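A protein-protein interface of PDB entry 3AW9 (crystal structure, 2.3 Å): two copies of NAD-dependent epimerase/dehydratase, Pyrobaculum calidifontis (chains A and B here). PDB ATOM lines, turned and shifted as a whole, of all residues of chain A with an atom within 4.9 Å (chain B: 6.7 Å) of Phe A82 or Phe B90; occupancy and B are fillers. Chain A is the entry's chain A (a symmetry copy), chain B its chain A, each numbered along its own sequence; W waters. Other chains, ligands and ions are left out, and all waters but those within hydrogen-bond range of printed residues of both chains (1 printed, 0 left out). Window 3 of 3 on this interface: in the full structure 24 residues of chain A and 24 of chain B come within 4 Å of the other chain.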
ATOM      1  N   PRO A  78     -18.372  26.064   8.182  1.00  0.00           N
ATOM      2  CA  PRO A  78     -19.014  24.940   8.909  1.00  0.00           C
ATOM      3  C   PRO A  78     -18.778  23.531   8.321  1.00  0.00           C
ATOM      4  O   PRO A  78     -18.885  22.546   9.065  1.00  0.00           O
ATOM      5  CB  PRO A  78     -20.513  25.295   8.868  1.00  0.00           C
ATOM      6  CG  PRO A  78     -20.552  26.795   8.664  1.00  0.00           C
ATOM      7  CD  PRO A  78     -19.368  27.077   7.770  1.00  0.00           C
ATOM      8  N   ILE A  79     -18.468  23.461   7.017  1.00  0.00           N
ATOM      9  CA  ILE A  79     -18.229  22.205   6.315  1.00  0.00           C
ATOM     10  C   ILE A  79     -16.969  21.480   6.797  1.00  0.00           C
ATOM     11  O   ILE A  79     -16.929  20.245   6.851  1.00  0.00           O
ATOM     12  CB  ILE A  79     -18.185  22.404   4.782  1.00  0.00           C
ATOM     13  CG1 ILE A  79     -18.024  21.065   4.066  1.00  0.00           C
ATOM     14  CG2 ILE A  79     -17.082  23.379   4.373  1.00  0.00           C
ATOM     15  CD1 ILE A  79     -18.049  21.189   2.569  1.00  0.00           C
ATOM     16  N   VAL A  80     -15.946  22.267   7.138  1.00  0.00           N
ATOM     17  CA  VAL A  80     -14.686  21.759   7.653  1.00  0.00           C
ATOM     18  C   VAL A  80     -14.978  21.196   9.016  1.00  0.00           C
ATOM     19  O   VAL A  80     -14.604  20.064   9.300  1.00  0.00           O
ATOM     20  CB  VAL A  80     -13.566  22.866   7.662  1.00  0.00           C
ATOM     21  CG1 VAL A  80     -12.579  22.700   8.834  1.00  0.00           C
ATOM     22  CG2 VAL A  80     -12.801  22.858   6.322  1.00  0.00           C
ATOM     23  N   HIS A  81     -15.696  21.961   9.843  1.00  0.00           N
ATOM     24  CA  HIS A  81     -16.184  21.430  11.104  1.00  0.00           C
ATOM     25  C   HIS A  81     -17.000  20.168  10.907  1.00  0.00           C
ATOM     26  O   HIS A  81     -16.991  19.292  11.780  1.00  0.00           O
ATOM     27  CB  HIS A  81     -17.046  22.430  11.881  1.00  0.00           C
ATOM     28  CG  HIS A  81     -16.264  23.429  12.673  1.00  0.00           C
ATOM     29  ND1 HIS A  81     -16.783  24.655  13.031  1.00  0.00           N
ATOM     30  CD2 HIS A  81     -14.989  23.405  13.140  1.00  0.00           C
ATOM     31  CE1 HIS A  81     -15.866  25.336  13.700  1.00  0.00           C
ATOM     32  NE2 HIS A  81     -14.771  24.596  13.786  1.00  0.00           N
ATOM     33  N   PHE A  82     -17.730  20.084   9.789  1.00  0.00           N
ATOM     34  CA  PHE A  82     -18.698  19.019   9.630  1.00  0.00           C
ATOM     35  C   PHE A  82     -17.954  17.730   9.360  1.00  0.00           C
ATOM     36  O   PHE A  82     -18.180  16.758  10.029  1.00  0.00           O
ATOM     37  CB  PHE A  82     -19.735  19.307   8.525  1.00  0.00           C
ATOM     38  CG  PHE A  82     -20.746  18.216   8.387  1.00  0.00           C
ATOM     39  CD1 PHE A  82     -21.753  18.080   9.320  1.00  0.00           C
ATOM     40  CD2 PHE A  82     -20.662  17.285   7.363  1.00  0.00           C
ATOM     41  CE1 PHE A  82     -22.688  17.053   9.237  1.00  0.00           C
ATOM     42  CE2 PHE A  82     -21.613  16.236   7.282  1.00  0.00           C
ATOM     43  CZ  PHE A  82     -22.617  16.130   8.240  1.00  0.00           C
ATOM     44  N   ASN A  83     -17.063  17.760   8.376  1.00  0.00           N
ATOM     45  CA  ASN A  83     -16.248  16.632   8.021  1.00  0.00           C
ATOM     46  C   ASN A  83     -15.264  16.179   9.106  1.00  0.00           C
ATOM     47  O   ASN A  83     -15.111  14.979   9.339  1.00  0.00           O
ATOM     48  CB  ASN A  83     -15.462  16.951   6.753  1.00  0.00           C
ATOM     49  CG  ASN A  83     -16.322  16.992   5.536  1.00  0.00           C
ATOM     50  OD1 ASN A  83     -17.503  16.649   5.578  1.00  0.00           O
ATOM     51  ND2 ASN A  83     -15.725  17.402   4.410  1.00  0.00           N
ATOM     52  N   GLU A  84     -14.604  17.149   9.732  1.00  0.00           N
ATOM     53  CA  GLU A  84     -13.599  16.924  10.758  1.00  0.00           C
ATOM     54  C   GLU A  84     -14.198  16.404  12.055  1.00  0.00           C
ATOM     55  O   GLU A  84     -13.601  15.574  12.734  1.00  0.00           O
ATOM     56  CB  GLU A  84     -12.867  18.247  11.050  1.00  0.00           C
ATOM     57  CG  GLU A  84     -11.761  18.510  10.104  1.00  0.00           C
ATOM     58  CD  GLU A  84     -10.605  17.548  10.338  1.00  0.00           C
ATOM     59  OE1 GLU A  84      -9.945  17.631  11.424  1.00  0.00           O
ATOM     60  OE2 GLU A  84     -10.376  16.720   9.438  1.00  0.00           O
ATOM     61  N   ASN A  85     -15.388  16.904  12.375  1.00  0.00           N
ATOM     62  CA  ASN A  85     -15.987  16.656  13.665  1.00  0.00           C
ATOM     63  C   ASN A  85     -17.159  15.673  13.629  1.00  0.00           C
ATOM     64  O   ASN A  85     -17.335  14.920  14.588  1.00  0.00           O
ATOM     65  CB  ASN A  85     -16.351  17.977  14.365  1.00  0.00           C
ATOM     66  CG  ASN A  85     -15.110  18.821  14.713  1.00  0.00           C
ATOM     67  OD1 ASN A  85     -13.981  18.311  14.782  1.00  0.00           O
ATOM     68  ND2 ASN A  85     -15.316  20.106  14.943  1.00  0.00           N
ATOM     69  N   VAL A  86     -17.903  15.625  12.518  1.00  0.00           N
ATOM     70  CA  VAL A  86     -19.088  14.769  12.409  1.00  0.00           C
ATOM     71  C   VAL A  86     -18.832  13.523  11.562  1.00  0.00           C
ATOM     72  O   VAL A  86     -19.082  12.420  12.020  1.00  0.00           O
ATOM     73  CB  VAL A  86     -20.369  15.550  11.893  1.00  0.00           C
ATOM     74  CG1 VAL A  86     -21.612  14.686  11.994  1.00  0.00           C
ATOM     75  CG2 VAL A  86     -20.583  16.824  12.687  1.00  0.00           C
ATOM     76  N   VAL A  87     -18.385  13.698  10.320  1.00  0.00           N
ATOM     77  CA  VAL A  87     -18.121  12.562   9.432  1.00  0.00           C
ATOM     78  C   VAL A  87     -17.015  11.685  10.008  1.00  0.00           C
ATOM     79  O   VAL A  87     -17.157  10.466  10.038  1.00  0.00           O
ATOM     80  CB  VAL A  87     -17.801  13.009   7.952  1.00  0.00           C
ATOM     81  CG1 VAL A  87     -17.531  11.808   7.047  1.00  0.00           C
ATOM     82  CG2 VAL A  87     -18.963  13.794   7.389  1.00  0.00           C
ATOM     83  N   LEU B  48     -29.838  15.758  -2.568  1.00  0.00           N
ATOM     84  CA  LEU B  48     -29.404  16.505  -1.373  1.00  0.00           C
ATOM     85  C   LEU B  48     -28.101  16.040  -0.695  1.00  0.00           C
ATOM     86  O   LEU B  48     -27.519  16.780   0.115  1.00  0.00           O
ATOM     87  CB  LEU B  48     -30.556  16.567  -0.368  1.00  0.00           C
ATOM     88  CG  LEU B  48     -31.549  17.733  -0.534  1.00  0.00           C
ATOM     89  CD1 LEU B  48     -32.180  17.748  -1.935  1.00  0.00           C
ATOM     90  CD2 LEU B  48     -32.613  17.670   0.511  1.00  0.00           C
ATOM     91  N   TYR B  51     -23.619  18.706  -2.059  1.00  0.00           N
ATOM     92  CA  TYR B  51     -23.556  20.024  -1.430  1.00  0.00           C
ATOM     93  C   TYR B  51     -24.201  21.090  -2.318  1.00  0.00           C
ATOM     94  O   TYR B  51     -24.891  21.975  -1.835  1.00  0.00           O
ATOM     95  CB  TYR B  51     -22.115  20.386  -1.094  1.00  0.00           C
ATOM     96  CG  TYR B  51     -21.966  21.638  -0.252  1.00  0.00           C
ATOM     97  CD1 TYR B  51     -22.310  21.652   1.120  1.00  0.00           C
ATOM     98  CD2 TYR B  51     -21.463  22.815  -0.816  1.00  0.00           C
ATOM     99  CE1 TYR B  51     -22.153  22.792   1.889  1.00  0.00           C
ATOM    100  CE2 TYR B  51     -21.306  23.977  -0.043  1.00  0.00           C
ATOM    101  CZ  TYR B  51     -21.647  23.957   1.306  1.00  0.00           C
ATOM    102  OH  TYR B  51     -21.477  25.120   2.041  1.00  0.00           O
ATOM    103  N   TRP B  53     -26.674  20.870  -4.387  1.00  0.00           N
ATOM    104  CA  TRP B  53     -28.064  20.529  -4.784  1.00  0.00           C
ATOM    105  C   TRP B  53     -28.983  21.730  -5.027  1.00  0.00           C
ATOM    106  O   TRP B  53     -29.887  21.666  -5.877  1.00  0.00           O
ATOM    107  CB  TRP B  53     -28.754  19.605  -3.749  1.00  0.00           C
ATOM    108  CG  TRP B  53     -29.094  20.336  -2.455  1.00  0.00           C
ATOM    109  CD1 TRP B  53     -28.279  20.491  -1.364  1.00  0.00           C
ATOM    110  CD2 TRP B  53     -30.309  21.034  -2.142  1.00  0.00           C
ATOM    111  NE1 TRP B  53     -28.910  21.234  -0.400  1.00  0.00           N
ATOM    112  CE2 TRP B  53     -30.155  21.584  -0.852  1.00  0.00           C
ATOM    113  CE3 TRP B  53     -31.513  21.245  -2.825  1.00  0.00           C
ATOM    114  CZ2 TRP B  53     -31.153  22.337  -0.233  1.00  0.00           C
ATOM    115  CZ3 TRP B  53     -32.525  21.997  -2.191  1.00  0.00           C
ATOM    116  CH2 TRP B  53     -32.326  22.529  -0.912  1.00  0.00           C
ATOM    117  N   HIS B  64     -38.094  20.425   5.151  1.00  0.00           N
ATOM    118  CA  HIS B  64     -37.107  19.412   4.791  1.00  0.00           C
ATOM    119  C   HIS B  64     -37.573  18.016   5.156  1.00  0.00           C
ATOM    120  O   HIS B  64     -37.517  17.592   6.325  1.00  0.00           O
ATOM    121  CB  HIS B  64     -35.716  19.742   5.345  1.00  0.00           C
ATOM    122  CG  HIS B  64     -34.721  18.636   5.184  1.00  0.00           C
ATOM    123  ND1 HIS B  64     -34.486  18.018   3.972  1.00  0.00           N
ATOM    124  CD2 HIS B  64     -33.921  18.020   6.085  1.00  0.00           C
ATOM    125  CE1 HIS B  64     -33.579  17.068   4.134  1.00  0.00           C
ATOM    126  NE2 HIS B  64     -33.213  17.057   5.404  1.00  0.00           N
ATOM    127  N   PHE B  82     -26.437   7.635   6.962  1.00  0.00           N
ATOM    128  CA  PHE B  82     -25.631   8.744   7.430  1.00  0.00           C
ATOM    129  C   PHE B  82     -25.682   9.845   6.394  1.00  0.00           C
ATOM    130  O   PHE B  82     -25.985  10.961   6.721  1.00  0.00           O
ATOM    131  CB  PHE B  82     -24.177   8.343   7.748  1.00  0.00           C
ATOM    132  CG  PHE B  82     -23.363   9.487   8.257  1.00  0.00           C
ATOM    133  CD1 PHE B  82     -23.536   9.944   9.546  1.00  0.00           C
ATOM    134  CD2 PHE B  82     -22.466  10.152   7.434  1.00  0.00           C
ATOM    135  CE1 PHE B  82     -22.817  11.030  10.036  1.00  0.00           C
ATOM    136  CE2 PHE B  82     -21.738  11.262   7.934  1.00  0.00           C
ATOM    137  CZ  PHE B  82     -21.937  11.694   9.242  1.00  0.00           C
ATOM    138  N   ASN B  85     -29.499  11.011   5.733  1.00  0.00           N
ATOM    139  CA  ASN B  85     -30.181  11.607   6.857  1.00  0.00           C
ATOM    140  C   ASN B  85     -29.371  12.689   7.575  1.00  0.00           C
ATOM    141  O   ASN B  85     -29.965  13.650   8.065  1.00  0.00           O
ATOM    142  CB  ASN B  85     -30.700  10.526   7.821  1.00  0.00           C
ATOM    143  CG  ASN B  85     -31.787   9.640   7.182  1.00  0.00           C
ATOM    144  OD1 ASN B  85     -32.424  10.016   6.186  1.00  0.00           O
ATOM    145  ND2 ASN B  85     -32.009   8.471   7.757  1.00  0.00           N
ATOM    146  N   VAL B  86     -28.038  12.576   7.577  1.00  0.00           N
ATOM    147  CA  VAL B  86     -27.177  13.520   8.294  1.00  0.00           C
ATOM    148  C   VAL B  86     -26.485  14.509   7.357  1.00  0.00           C
ATOM    149  O   VAL B  86     -26.586  15.707   7.562  1.00  0.00           O
ATOM    150  CB  VAL B  86     -26.122  12.800   9.235  1.00  0.00           C
ATOM    151  CG1 VAL B  86     -25.396  13.805  10.111  1.00  0.00           C
ATOM    152  CG2 VAL B  86     -26.797  11.768  10.117  1.00  0.00           C
ATOM    153  N   VAL B  87     -25.746  14.012   6.365  1.00  0.00           N
ATOM    154  CA  VAL B  87     -25.039  14.883   5.424  1.00  0.00           C
ATOM    155  C   VAL B  87     -26.033  15.730   4.637  1.00  0.00           C
ATOM    156  O   VAL B  87     -25.833  16.933   4.499  1.00  0.00           O
ATOM    157  CB  VAL B  87     -24.066  14.085   4.470  1.00  0.00           C
ATOM    158  CG1 VAL B  87     -23.340  15.016   3.500  1.00  0.00           C
ATOM    159  CG2 VAL B  87     -23.041  13.337   5.290  1.00  0.00           C
ATOM    160  N   ALA B  88     -27.106  15.108   4.147  1.00  0.00           N
ATOM    161  CA  ALA B  88     -28.174  15.801   3.395  1.00  0.00           C
ATOM    162  C   ALA B  88     -28.857  16.952   4.160  1.00  0.00           C
ATOM    163  O   ALA B  88     -29.118  18.034   3.595  1.00  0.00           O
ATOM    164  CB  ALA B  88     -29.219  14.793   2.956  1.00  0.00           C
ATOM    165  N   THR B  89     -29.151  16.718   5.436  1.00  0.00           N
ATOM    166  CA  THR B  89     -29.720  17.739   6.326  1.00  0.00           C
ATOM    167  C   THR B  89     -28.716  18.890   6.518  1.00  0.00           C
ATOM    168  O   THR B  89     -29.053  20.084   6.394  1.00  0.00           O
ATOM    169  CB  THR B  89     -30.087  17.064   7.673  1.00  0.00           C
ATOM    170  OG1 THR B  89     -31.099  16.088   7.424  1.00  0.00           O
ATOM    171  CG2 THR B  89     -30.548  18.079   8.765  1.00  0.00           C
ATOM    172  N   PHE B  90     -27.460  18.536   6.775  1.00  0.00           N
ATOM    173  CA  PHE B  90     -26.426  19.558   6.806  1.00  0.00           C
ATOM    174  C   PHE B  90     -26.374  20.344   5.480  1.00  0.00           C
ATOM    175  O   PHE B  90     -26.222  21.548   5.494  1.00  0.00           O
ATOM    176  CB  PHE B  90     -25.053  18.970   7.183  1.00  0.00           C
ATOM    177  CG  PHE B  90     -23.925  19.957   7.047  1.00  0.00           C
ATOM    178  CD1 PHE B  90     -23.701  20.924   8.034  1.00  0.00           C
ATOM    179  CD2 PHE B  90     -23.090  19.932   5.932  1.00  0.00           C
ATOM    180  CE1 PHE B  90     -22.643  21.870   7.908  1.00  0.00           C
ATOM    181  CE2 PHE B  90     -22.043  20.866   5.803  1.00  0.00           C
ATOM    182  CZ  PHE B  90     -21.819  21.826   6.814  1.00  0.00           C
ATOM    183  N   ASN B  91     -26.466  19.663   4.344  1.00  0.00           N
ATOM    184  CA  ASN B  91     -26.418  20.337   3.045  1.00  0.00           C
ATOM    185  C   ASN B  91     -27.637  21.258   2.863  1.00  0.00           C
ATOM    186  O   ASN B  91     -27.530  22.318   2.256  1.00  0.00           O
ATOM    187  CB  ASN B  91     -26.393  19.330   1.882  1.00  0.00           C
ATOM    188  CG  ASN B  91     -25.048  18.569   1.734  1.00  0.00           C
ATOM    189  OD1 ASN B  91     -24.030  18.946   2.290  1.00  0.00           O
ATOM    190  ND2 ASN B  91     -25.065  17.505   0.934  1.00  0.00           N
ATOM    191  N   VAL B  92     -28.798  20.852   3.382  1.00  0.00           N
ATOM    192  CA  VAL B  92     -29.992  21.709   3.354  1.00  0.00           C
ATOM    193  C   VAL B  92     -29.789  22.972   4.188  1.00  0.00           C
ATOM    194  O   VAL B  92     -30.082  24.080   3.722  1.00  0.00           O
ATOM    195  CB  VAL B  92     -31.278  20.950   3.810  1.00  0.00           C
ATOM    196  CG1 VAL B  92     -32.492  21.892   3.863  1.00  0.00           C
ATOM    197  CG2 VAL B  92     -31.577  19.807   2.847  1.00  0.00           C
ATOM    198  N   LEU B  93     -29.271  22.798   5.403  1.00  0.00           N
ATOM    199  CA  LEU B  93     -29.028  23.903   6.333  1.00  0.00           C
ATOM    200  C   LEU B  93     -27.976  24.877   5.831  1.00  0.00           C
ATOM    201  O   LEU B  93     -28.069  26.079   6.067  1.00  0.00           O
ATOM    202  CB  LEU B  93     -28.622  23.378   7.707  1.00  0.00           C
ATOM    203  CG  LEU B  93     -29.646  22.563   8.510  1.00  0.00           C
ATOM    204  CD1 LEU B  93     -28.911  21.846   9.621  1.00  0.00           C
ATOM    205  CD2 LEU B  93     -30.807  23.416   9.089  1.00  0.00           C
ATOM    206  N   GLU B  94     -26.972  24.366   5.135  1.00  0.00           N
ATOM    207  CA  GLU B  94     -25.984  25.235   4.505  1.00  0.00           C
ATOM    208  C   GLU B  94     -26.588  26.011   3.329  1.00  0.00           C
ATOM    209  O   GLU B  94     -26.298  27.174   3.149  1.00  0.00           O
ATOM    210  CB  GLU B  94     -24.754  24.436   4.080  1.00  0.00           C
ATOM    211  CG  GLU B  94     -23.727  24.305   5.173  1.00  0.00           C
ATOM    212  CD  GLU B  94     -23.053  25.635   5.505  1.00  0.00           C
ATOM    213  OE1 GLU B  94     -23.361  26.246   6.551  1.00  0.00           O
ATOM    214  OE2 GLU B  94     -22.228  26.084   4.697  1.00  0.00           O
ATOM    215  N   TRP B  95     -27.435  25.377   2.532  1.00  0.00           N
ATOM    216  CA  TRP B  95     -28.159  26.111   1.496  1.00  0.00           C
ATOM    217  C   TRP B  95     -29.060  27.199   2.096  1.00  0.00           C
ATOM    218  O   TRP B  95     -29.075  28.320   1.599  1.00  0.00           O
ATOM    219  CB  TRP B  95     -28.967  25.139   0.633  1.00  0.00           C
ATOM    220  CG  TRP B  95     -30.084  25.756  -0.169  1.00  0.00           C
ATOM    221  CD1 TRP B  95     -30.005  26.283  -1.430  1.00  0.00           C
ATOM    222  CD2 TRP B  95     -31.447  25.885   0.236  1.00  0.00           C
ATOM    223  NE1 TRP B  95     -31.236  26.727  -1.837  1.00  0.00           N
ATOM    224  CE2 TRP B  95     -32.139  26.497  -0.831  1.00  0.00           C
ATOM    225  CE3 TRP B  95     -32.161  25.530   1.403  1.00  0.00           C
ATOM    226  CZ2 TRP B  95     -33.502  26.760  -0.767  1.00  0.00           C
ATOM    227  CZ3 TRP B  95     -33.493  25.786   1.458  1.00  0.00           C
ATOM    228  CH2 TRP B  95     -34.161  26.412   0.389  1.00  0.00           C
ATOM    229  N   GLY B 140     -29.689  15.823  13.196  1.00  0.00           N
ATOM    230  CA  GLY B 140     -30.379  16.830  12.398  1.00  0.00           C
ATOM    231  C   GLY B 140     -31.052  17.902  13.231  1.00  0.00           C
ATOM    232  O   GLY B 140     -30.895  19.090  12.951  1.00  0.00           O
ATOM    233  N   MET B 143     -28.383  20.192  14.846  1.00  0.00           N
ATOM    234  CA  MET B 143     -27.769  21.055  13.840  1.00  0.00           C
ATOM    235  C   MET B 143     -28.718  22.177  13.425  1.00  0.00           C
ATOM    236  O   MET B 143     -28.274  23.321  13.287  1.00  0.00           O
ATOM    237  CB  MET B 143     -27.319  20.282  12.584  1.00  0.00           C
ATOM    238  CG  MET B 143     -26.181  19.255  12.753  1.00  0.00           C
ATOM    239  SD  MET B 143     -25.540  18.482  11.181  1.00  0.00           S
ATOM    240  CE  MET B 143     -26.950  17.518  10.595  1.00  0.00           C
ATOM    241  N   TYR B 147     -28.200  26.236  13.915  1.00  0.00           N
ATOM    242  CA  TYR B 147     -28.328  27.177  12.821  1.00  0.00           C
ATOM    243  C   TYR B 147     -29.347  28.266  13.136  1.00  0.00           C
ATOM    244  O   TYR B 147     -29.174  29.404  12.706  1.00  0.00           O
ATOM    245  CB  TYR B 147     -28.677  26.460  11.495  1.00  0.00           C
ATOM    246  CG  TYR B 147     -27.446  26.007  10.742  1.00  0.00           C
ATOM    247  CD1 TYR B 147     -26.547  25.086  11.304  1.00  0.00           C
ATOM    248  CD2 TYR B 147     -27.164  26.505   9.488  1.00  0.00           C
ATOM    249  CE1 TYR B 147     -25.407  24.665  10.606  1.00  0.00           C
ATOM    250  CE2 TYR B 147     -26.020  26.102   8.781  1.00  0.00           C
ATOM    251  CZ  TYR B 147     -25.151  25.189   9.349  1.00  0.00           C
ATOM    252  OH  TYR B 147     -24.037  24.836   8.643  1.00  0.00           O
HETATM  253  O   HOH W   1     -19.352  25.452   5.379  1.00  0.00           O
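Water W1 bridges the backbone NH of Ile A79 (2.7 Å) and the side-chain carboxylate of Glu B94 (3.0 Å).
Phe A82 touches Val B87, and with the chains exchanged Val A87 touches Phe B82. Of the 8 pairs that touch across the chains among the printed residues, 2 have their exchanged pair printed and touching as well.
Printed residues of chain B within 4 Å of Pro A78: Phe B90 (3.8 Å), Glu B94 (3.6 Å) and Tyr B147 (3.6 Å). Phe A82 touches three residues of chain B. Printed residues of chain B within 4 Å of Val A87: Phe B82 (3.8 Å). Trp B53 touches none of the printed residues of chain A. Printed residues of chain A within 4 Å of Val B87: Phe A82 (3.8 Å). Of chain A, only Pro A78 (3.8 Å), Ile A79 (3.6 Å) and Phe A82 (3.7 Å) come within 4 Å of Phe B90. Printed residues of chain A within 4 Å of Glu B94: Pro A78 (3.6 Å). The nearest residue of chain B that does not touch Phe A82 is Val B86 (4.05 Å).
Printed residues of chain B that touch a printed residue of chain A: Phe B82, Val B87, Phe B90, Glu B94, Met B143 and Tyr B147. Of the 10 printed residues of chain A, 4 touch a printed residue of chain B. Hydrophobic or aromatic side chains of chain A within 4 Å of the printed part of chain B: Pro A78, Phe A82 and Val A87. Among the printed residues, 8 pairs touch across the chains.
Among the printed residues, merely in contact across the chains: Pro A78 with Phe B90, Pro A78 with Glu B94, Pro A78 with Tyr B147, Ile A79 with Phe B90, Phe A82 with Val B87, Phe A82 with Phe B90, Phe A82 with Met B143 and Val A87 with Phe B82.
O of Phe B82 is in hydrogen-bond range of N of Val B87, at 3.1 Å. The side-chain carboxylate of Glu B94 lies within hydrogen-bond range of the side-chain hydroxyl of Tyr B147, 2.6 Å away. The backbone carbonyl oxygen (O) of Phe A82 is in hydrogen-bond range of the backbone NH (N) of Val A87 (3.1 Å). OH of Tyr B51 sits at hydrogen-bond distance from OE2 of Glu B94, at 2.9 Å. The backbone carbonyl oxygen (O) of Val B87 lies close to the side-chain amide oxygen (OD1) of Asn B91.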
